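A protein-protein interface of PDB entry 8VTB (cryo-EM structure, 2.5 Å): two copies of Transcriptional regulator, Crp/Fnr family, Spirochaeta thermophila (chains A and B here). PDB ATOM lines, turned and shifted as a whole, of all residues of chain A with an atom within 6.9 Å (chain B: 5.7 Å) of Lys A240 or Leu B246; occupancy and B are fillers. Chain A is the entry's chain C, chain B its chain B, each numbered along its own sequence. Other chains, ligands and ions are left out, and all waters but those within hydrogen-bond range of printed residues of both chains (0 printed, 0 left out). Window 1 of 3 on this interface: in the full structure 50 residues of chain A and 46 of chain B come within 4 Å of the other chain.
NZ of Lys A240 sits at hydrogen-bond distance from O of Ser B239.
O of Ser A236 lies within hydrogen-bond range of OG of Ser A239 (3.0 Å).
Among the printed residues, merely in contact across the chains: Pro A148 with Asp B242 (3.4 Å), Pro A148 with Lys B245 (3.7 Å), Pro A148 with Arg B249 (3.5 Å), Ser A236 with Ser B239 (3.4 Å) and Lys A240 with Leu B246 (3.7 Å).
Lys A240 touches just these residues of chain B: Ser B239 and Leu B246. Leu B246 touches one residue of chain A. Of the printed residues of chain A, Ser B239 touches Ser A236 (3.4 Å) and Lys A240 (3.3 Å). Of the printed residues of chain A, Asp B242 touches Pro A148. Of the printed residues of chain B, Ser A236 touches Ser B239. Ala A235 touches none of the printed residues of chain B. The nearest residue of chain B that does not touch Lys A240 is Lys B240 (5.5 Å). The nearest printed residue of chain B that does not touch Pro A148 is Leu B246 (4.7 Å).
Printed residues of chain A that touch a printed residue of chain B: Pro A148, Ser A236 and Lys A240. Hydrophobic or aromatic side chains of chain A within 4 Å of the printed part of chain B: Pro A148. Of the 12 printed residues of chain B, 5 touch a printed residue of chain A. Printed residues of chain B that touch a printed residue of chain A: Ser B239, Asp B242, Lys B245, Leu B246 and Arg B249. Hydrophobic or aromatic side chains of chain B that line the printed part of chain A: Leu B246. Among the printed residues, 6 pairs touch across the chains. Among the printed residues, no Asp or Glu carboxylate lies within 4 Å of a Lys or Arg side-chain nitrogen of the other chain.
Lys A240 touches Ser B239, but with the chains exchanged Ser A239 does not touch Lys B240 (8.5 Å). Lys A240 touches Leu B246, but with the chains exchanged Leu A246 does not touch Lys B240 (15.6 Å). Positions printed for both chains: 239, 240, 242, 243, 244 and 246. Of the 6 pairs that touch across the chains among the printed residues, none has its exchanged pair printed and touching as well.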
ATOM      1  N   ASN A 147     -10.823  -8.552   9.191  1.00  0.00           N
ATOM      2  CA  ASN A 147     -11.168  -8.490   7.778  1.00  0.00           C
ATOM      3  C   ASN A 147     -12.559  -7.874   7.630  1.00  0.00           C
ATOM      4  O   ASN A 147     -13.506  -8.330   8.286  1.00  0.00           O
ATOM      5  CB  ASN A 147     -11.115  -9.902   7.181  1.00  0.00           C
ATOM      6  CG  ASN A 147     -11.524  -9.963   5.706  1.00  0.00           C
ATOM      7  OD1 ASN A 147     -12.094  -9.031   5.147  1.00  0.00           O
ATOM      8  ND2 ASN A 147     -11.212 -11.086   5.070  1.00  0.00           N
ATOM      9  N   PRO A 148     -12.720  -6.839   6.799  1.00  0.00           N
ATOM     10  CA  PRO A 148     -14.037  -6.190   6.665  1.00  0.00           C
ATOM     11  C   PRO A 148     -15.169  -7.130   6.283  1.00  0.00           C
ATOM     12  O   PRO A 148     -16.286  -6.971   6.793  1.00  0.00           O
ATOM     13  CB  PRO A 148     -13.788  -5.132   5.580  1.00  0.00           C
ATOM     14  CG  PRO A 148     -12.338  -4.821   5.685  1.00  0.00           C
ATOM     15  CD  PRO A 148     -11.663  -6.105   6.085  1.00  0.00           C
ATOM     16  N   ALA A 149     -14.924  -8.100   5.398  1.00  0.00           N
ATOM     17  CA  ALA A 149     -15.981  -9.040   5.040  1.00  0.00           C
ATOM     18  C   ALA A 149     -16.392  -9.886   6.241  1.00  0.00           C
ATOM     19  O   ALA A 149     -17.589 -10.083   6.495  1.00  0.00           O
ATOM     20  CB  ALA A 149     -15.523  -9.932   3.888  1.00  0.00           C
ATOM     21  N   ALA A 235     -20.192 -16.388   0.873  1.00  0.00           N
ATOM     22  CA  ALA A 235     -19.619 -16.580  -0.454  1.00  0.00           C
ATOM     23  C   ALA A 235     -18.565 -15.524  -0.752  1.00  0.00           C
ATOM     24  O   ALA A 235     -17.479 -15.838  -1.254  1.00  0.00           O
ATOM     25  CB  ALA A 235     -20.724 -16.556  -1.510  1.00  0.00           C
ATOM     26  N   SER A 236     -18.869 -14.260  -0.449  1.00  0.00           N
ATOM     27  CA  SER A 236     -17.904 -13.184  -0.643  1.00  0.00           C
ATOM     28  C   SER A 236     -16.642 -13.427   0.177  1.00  0.00           C
ATOM     29  O   SER A 236     -15.520 -13.270  -0.317  1.00  0.00           O
ATOM     30  CB  SER A 236     -18.540 -11.842  -0.281  1.00  0.00           C
ATOM     31  OG  SER A 236     -17.589 -10.794  -0.324  1.00  0.00           O
ATOM     32  N   LEU A 237     -16.815 -13.803   1.446  1.00  0.00           N
ATOM     33  CA  LEU A 237     -15.669 -14.054   2.314  1.00  0.00           C
ATOM     34  C   LEU A 237     -14.788 -15.172   1.768  1.00  0.00           C
ATOM     35  O   LEU A 237     -13.562 -15.029   1.682  1.00  0.00           O
ATOM     36  CB  LEU A 237     -16.151 -14.386   3.726  1.00  0.00           C
ATOM     37  CG  LEU A 237     -15.084 -14.726   4.766  1.00  0.00           C
ATOM     38  CD1 LEU A 237     -14.160 -13.543   4.991  1.00  0.00           C
ATOM     39  CD2 LEU A 237     -15.730 -15.161   6.070  1.00  0.00           C
ATOM     40  N   VAL A 238     -15.397 -16.301   1.393  1.00  0.00           N
ATOM     41  CA  VAL A 238     -14.610 -17.458   0.979  1.00  0.00           C
ATOM     42  C   VAL A 238     -14.053 -17.312  -0.432  1.00  0.00           C
ATOM     43  O   VAL A 238     -13.062 -17.973  -0.766  1.00  0.00           O
ATOM     44  CB  VAL A 238     -15.434 -18.756   1.097  1.00  0.00           C
ATOM     45  CG1 VAL A 238     -16.026 -18.889   2.492  1.00  0.00           C
ATOM     46  CG2 VAL A 238     -16.522 -18.799   0.039  1.00  0.00           C
ATOM     47  N   SER A 239     -14.653 -16.473  -1.278  1.00  0.00           N
ATOM     48  CA  SER A 239     -14.123 -16.287  -2.624  1.00  0.00           C
ATOM     49  C   SER A 239     -12.826 -15.493  -2.644  1.00  0.00           C
ATOM     50  O   SER A 239     -12.158 -15.458  -3.682  1.00  0.00           O
ATOM     51  CB  SER A 239     -15.164 -15.597  -3.505  1.00  0.00           C
ATOM     52  OG  SER A 239     -15.312 -14.234  -3.149  1.00  0.00           O
ATOM     53  N   LYS A 240     -12.455 -14.858  -1.532  1.00  0.00           N
ATOM     54  CA  LYS A 240     -11.280 -14.003  -1.462  1.00  0.00           C
ATOM     55  C   LYS A 240     -10.134 -14.628  -0.677  1.00  0.00           C
ATOM     56  O   LYS A 240      -9.088 -13.990  -0.527  1.00  0.00           O
ATOM     57  CB  LYS A 240     -11.657 -12.660  -0.830  1.00  0.00           C
ATOM     58  CG  LYS A 240     -12.504 -11.772  -1.723  1.00  0.00           C
ATOM     59  CD  LYS A 240     -12.955 -10.526  -0.982  1.00  0.00           C
ATOM     60  CE  LYS A 240     -14.435 -10.257  -1.201  1.00  0.00           C
ATOM     61  NZ  LYS A 240     -14.746  -9.887  -2.608  1.00  0.00           N
ATOM     62  N   LEU A 241     -10.304 -15.852  -0.173  1.00  0.00           N
ATOM     63  CA  LEU A 241      -9.336 -16.419   0.763  1.00  0.00           C
ATOM     64  C   LEU A 241      -7.983 -16.661   0.101  1.00  0.00           C
ATOM     65  O   LEU A 241      -6.942 -16.253   0.629  1.00  0.00           O
ATOM     66  CB  LEU A 241      -9.882 -17.718   1.355  1.00  0.00           C
ATOM     67  CG  LEU A 241     -10.972 -17.580   2.419  1.00  0.00           C
ATOM     68  CD1 LEU A 241     -11.583 -18.936   2.735  1.00  0.00           C
ATOM     69  CD2 LEU A 241     -10.422 -16.927   3.678  1.00  0.00           C
ATOM     70  N   ASP A 242      -7.973 -17.334  -1.050  1.00  0.00           N
ATOM     71  CA  ASP A 242      -6.742 -17.768  -1.699  1.00  0.00           C
ATOM     72  C   ASP A 242      -6.329 -16.856  -2.850  1.00  0.00           C
ATOM     73  O   ASP A 242      -5.850 -17.345  -3.879  1.00  0.00           O
ATOM     74  CB  ASP A 242      -6.881 -19.207  -2.192  1.00  0.00           C
ATOM     75  CG  ASP A 242      -7.084 -20.192  -1.058  1.00  0.00           C
ATOM     76  OD1 ASP A 242      -6.647 -19.898   0.072  1.00  0.00           O
ATOM     77  OD2 ASP A 242      -7.679 -21.264  -1.302  1.00  0.00           O
ATOM     78  N   ALA A 243      -6.508 -15.541  -2.696  1.00  0.00           N
ATOM     79  CA  ALA A 243      -6.268 -14.613  -3.799  1.00  0.00           C
ATOM     80  C   ALA A 243      -4.853 -14.745  -4.354  1.00  0.00           C
ATOM     81  O   ALA A 243      -4.658 -14.849  -5.571  1.00  0.00           O
ATOM     82  CB  ALA A 243      -6.529 -13.180  -3.337  1.00  0.00           C
ATOM     83  N   ALA A 244      -3.850 -14.752  -3.473  1.00  0.00           N
ATOM     84  CA  ALA A 244      -2.468 -14.849  -3.932  1.00  0.00           C
ATOM     85  C   ALA A 244      -2.201 -16.193  -4.599  1.00  0.00           C
ATOM     86  O   ALA A 244      -1.574 -16.260  -5.665  1.00  0.00           O
ATOM     87  CB  ALA A 244      -1.510 -14.629  -2.761  1.00  0.00           C
ATOM     88  N   LEU A 246      -4.370 -18.257  -5.980  1.00  0.00           N
ATOM     89  CA  LEU A 246      -5.100 -18.366  -7.237  1.00  0.00           C
ATOM     90  C   LEU A 246      -4.466 -17.508  -8.325  1.00  0.00           C
ATOM     91  O   LEU A 246      -4.435 -17.910  -9.492  1.00  0.00           O
ATOM     92  CB  LEU A 246      -6.566 -17.987  -7.033  1.00  0.00           C
ATOM     93  CG  LEU A 246      -7.370 -18.936  -6.142  1.00  0.00           C
ATOM     94  CD1 LEU A 246      -8.715 -18.331  -5.785  1.00  0.00           C
ATOM     95  CD2 LEU A 246      -7.549 -20.293  -6.808  1.00  0.00           C
ATOM     96  N   SER B 239     -20.492  -8.740  -2.497  1.00  0.00           N
ATOM     97  CA  SER B 239     -19.094  -8.987  -2.825  1.00  0.00           C
ATOM     98  C   SER B 239     -18.383  -7.751  -3.356  1.00  0.00           C
ATOM     99  O   SER B 239     -17.153  -7.762  -3.456  1.00  0.00           O
ATOM    100  CB  SER B 239     -18.989 -10.120  -3.846  1.00  0.00           C
ATOM    101  OG  SER B 239     -19.431  -9.699  -5.123  1.00  0.00           O
ATOM    102  N   LYS B 240     -19.120  -6.695  -3.695  1.00  0.00           N
ATOM    103  CA  LYS B 240     -18.556  -5.493  -4.289  1.00  0.00           C
ATOM    104  C   LYS B 240     -18.525  -4.311  -3.330  1.00  0.00           C
ATOM    105  O   LYS B 240     -18.089  -3.224  -3.725  1.00  0.00           O
ATOM    106  CB  LYS B 240     -19.355  -5.114  -5.540  1.00  0.00           C
ATOM    107  CG  LYS B 240     -19.140  -6.046  -6.720  1.00  0.00           C
ATOM    108  CD  LYS B 240     -20.066  -5.691  -7.870  1.00  0.00           C
ATOM    109  CE  LYS B 240     -20.733  -6.931  -8.443  1.00  0.00           C
ATOM    110  NZ  LYS B 240     -19.768  -7.841  -9.117  1.00  0.00           N
ATOM    111  N   ASP B 242     -16.867  -3.465  -0.387  1.00  0.00           N
ATOM    112  CA  ASP B 242     -15.617  -2.933   0.141  1.00  0.00           C
ATOM    113  C   ASP B 242     -14.479  -2.987  -0.875  1.00  0.00           C
ATOM    114  O   ASP B 242     -13.337  -3.277  -0.503  1.00  0.00           O
ATOM    115  CB  ASP B 242     -15.220  -3.679   1.414  1.00  0.00           C
ATOM    116  CG  ASP B 242     -16.221  -3.488   2.536  1.00  0.00           C
ATOM    117  OD1 ASP B 242     -16.920  -2.454   2.540  1.00  0.00           O
ATOM    118  OD2 ASP B 242     -16.304  -4.371   3.416  1.00  0.00           O
ATOM    119  N   ALA B 243     -14.771  -2.710  -2.149  1.00  0.00           N
ATOM    120  CA  ALA B 243     -13.772  -2.871  -3.203  1.00  0.00           C
ATOM    121  C   ALA B 243     -12.509  -2.064  -2.915  1.00  0.00           C
ATOM    122  O   ALA B 243     -11.391  -2.586  -3.002  1.00  0.00           O
ATOM    123  CB  ALA B 243     -14.369  -2.464  -4.549  1.00  0.00           C
ATOM    124  N   ALA B 244     -12.669  -0.787  -2.561  1.00  0.00           N
ATOM    125  CA  ALA B 244     -11.505   0.055  -2.295  1.00  0.00           C
ATOM    126  C   ALA B 244     -10.741  -0.432  -1.070  1.00  0.00           C
ATOM    127  O   ALA B 244      -9.504  -0.515  -1.086  1.00  0.00           O
ATOM    128  CB  ALA B 244     -11.941   1.509  -2.115  1.00  0.00           C
ATOM    129  N   LYS B 245     -11.461  -0.757   0.006  1.00  0.00           N
ATOM    130  CA  LYS B 245     -10.799  -1.203   1.228  1.00  0.00           C
ATOM    131  C   LYS B 245     -10.103  -2.541   1.020  1.00  0.00           C
ATOM    132  O   LYS B 245      -8.996  -2.757   1.524  1.00  0.00           O
ATOM    133  CB  LYS B 245     -11.812  -1.284   2.368  1.00  0.00           C
ATOM    134  CG  LYS B 245     -11.297  -1.974   3.616  1.00  0.00           C
ATOM    135  CD  LYS B 245     -11.302  -1.030   4.807  1.00  0.00           C
ATOM    136  CE  LYS B 245     -12.714  -0.776   5.308  1.00  0.00           C
ATOM    137  NZ  LYS B 245     -12.811   0.502   6.065  1.00  0.00           N
ATOM    138  N   LEU B 246     -10.726  -3.446   0.266  1.00  0.00           N
ATOM    139  CA  LEU B 246     -10.097  -4.735   0.006  1.00  0.00           C
ATOM    140  C   LEU B 246      -8.885  -4.589  -0.906  1.00  0.00           C
ATOM    141  O   LEU B 246      -7.886  -5.292  -0.725  1.00  0.00           O
ATOM    142  CB  LEU B 246     -11.112  -5.708  -0.594  1.00  0.00           C
ATOM    143  CG  LEU B 246     -12.254  -6.121   0.336  1.00  0.00           C
ATOM    144  CD1 LEU B 246     -13.336  -6.856  -0.431  1.00  0.00           C
ATOM    145  CD2 LEU B 246     -11.740  -6.970   1.491  1.00  0.00           C
ATOM    146  N   LEU B 247      -8.950  -3.685  -1.887  1.00  0.00           N
ATOM    147  CA  LEU B 247      -7.773  -3.412  -2.708  1.00  0.00           C
ATOM    148  C   LEU B 247      -6.635  -2.854  -1.866  1.00  0.00           C
ATOM    149  O   LEU B 247      -5.477  -3.268  -2.017  1.00  0.00           O
ATOM    150  CB  LEU B 247      -8.128  -2.442  -3.833  1.00  0.00           C
ATOM    151  CG  LEU B 247      -8.850  -3.032  -5.040  1.00  0.00           C
ATOM    152  CD1 LEU B 247      -9.289  -1.927  -5.985  1.00  0.00           C
ATOM    153  CD2 LEU B 247      -7.945  -4.022  -5.747  1.00  0.00           C
ATOM    154  N   HIS B 248      -6.946  -1.923  -0.962  1.00  0.00           N
ATOM    155  CA  HIS B 248      -5.919  -1.372  -0.088  1.00  0.00           C
ATOM    156  C   HIS B 248      -5.320  -2.459   0.796  1.00  0.00           C
ATOM    157  O   HIS B 248      -4.098  -2.529   0.972  1.00  0.00           O
ATOM    158  CB  HIS B 248      -6.505  -0.245   0.760  1.00  0.00           C
ATOM    159  CG  HIS B 248      -5.488   0.498   1.569  1.00  0.00           C
ATOM    160  ND1 HIS B 248      -4.610   1.404   1.012  1.00  0.00           N
ATOM    161  CD2 HIS B 248      -5.205   0.468   2.893  1.00  0.00           C
ATOM    162  CE1 HIS B 248      -3.833   1.901   1.959  1.00  0.00           C
ATOM    163  NE2 HIS B 248      -4.175   1.349   3.109  1.00  0.00           N
ATOM    164  N   ARG B 249      -6.170  -3.326   1.353  1.00  0.00           N
ATOM    165  CA  ARG B 249      -5.681  -4.401   2.209  1.00  0.00           C
ATOM    166  C   ARG B 249      -4.801  -5.377   1.440  1.00  0.00           C
ATOM    167  O   ARG B 249      -3.759  -5.807   1.945  1.00  0.00           O
ATOM    168  CB  ARG B 249      -6.853  -5.133   2.853  1.00  0.00           C
ATOM    169  CG  ARG B 249      -7.397  -4.453   4.090  1.00  0.00           C
ATOM    170  CD  ARG B 249      -8.509  -5.276   4.694  1.00  0.00           C
ATOM    171  NE  ARG B 249      -8.059  -6.621   5.039  1.00  0.00           N
ATOM    172  CZ  ARG B 249      -7.511  -6.953   6.200  1.00  0.00           C
ATOM    173  NH1 ARG B 249      -7.334  -6.062   7.161  1.00  0.00           N
ATOM    174  NH2 ARG B 249      -7.134  -8.213   6.400  1.00  0.00           N
ATOM    175  N   GLU B 250      -5.204  -5.758   0.227  1.00  0.00           N
ATOM    176  CA  GLU B 250      -4.379  -6.684  -0.542  1.00  0.00           C
ATOM    177  C   GLU B 250      -3.050  -6.040  -0.915  1.00  0.00           C
ATOM    178  O   GLU B 250      -2.010  -6.706  -0.874  1.00  0.00           O
ATOM    179  CB  GLU B 250      -5.174  -7.204  -1.755  1.00  0.00           C
ATOM    180  CG  GLU B 250      -5.462  -6.270  -2.956  1.00  0.00           C
ATOM    181  CD  GLU B 250      -4.249  -5.810  -3.753  1.00  0.00           C
ATOM    182  OE1 GLU B 250      -3.178  -6.446  -3.665  1.00  0.00           O
ATOM    183  OE2 GLU B 250      -4.371  -4.801  -4.480  1.00  0.00           O
ATOM    184  N   ARG B 251      -3.060  -4.742  -1.228  1.00  0.00           N
ATOM    185  CA  ARG B 251      -1.816  -4.026  -1.492  1.00  0.00           C
ATOM    186  C   ARG B 251      -0.901  -4.047  -0.271  1.00  0.00           C
ATOM    187  O   ARG B 251       0.294  -4.350  -0.377  1.00  0.00           O
ATOM    188  CB  ARG B 251      -2.141  -2.591  -1.908  1.00  0.00           C
ATOM    189  CG  ARG B 251      -0.953  -1.662  -2.042  1.00  0.00           C
ATOM    190  CD  ARG B 251      -1.402  -0.314  -2.589  1.00  0.00           C
ATOM    191  NE  ARG B 251      -0.302   0.628  -2.742  1.00  0.00           N
ATOM    192  CZ  ARG B 251      -0.422   1.838  -3.271  1.00  0.00           C
ATOM    193  NH1 ARG B 251      -1.587   2.286  -3.711  1.00  0.00           N
ATOM    194  NH2 ARG B 251       0.651   2.622  -3.353  1.00  0.00           N
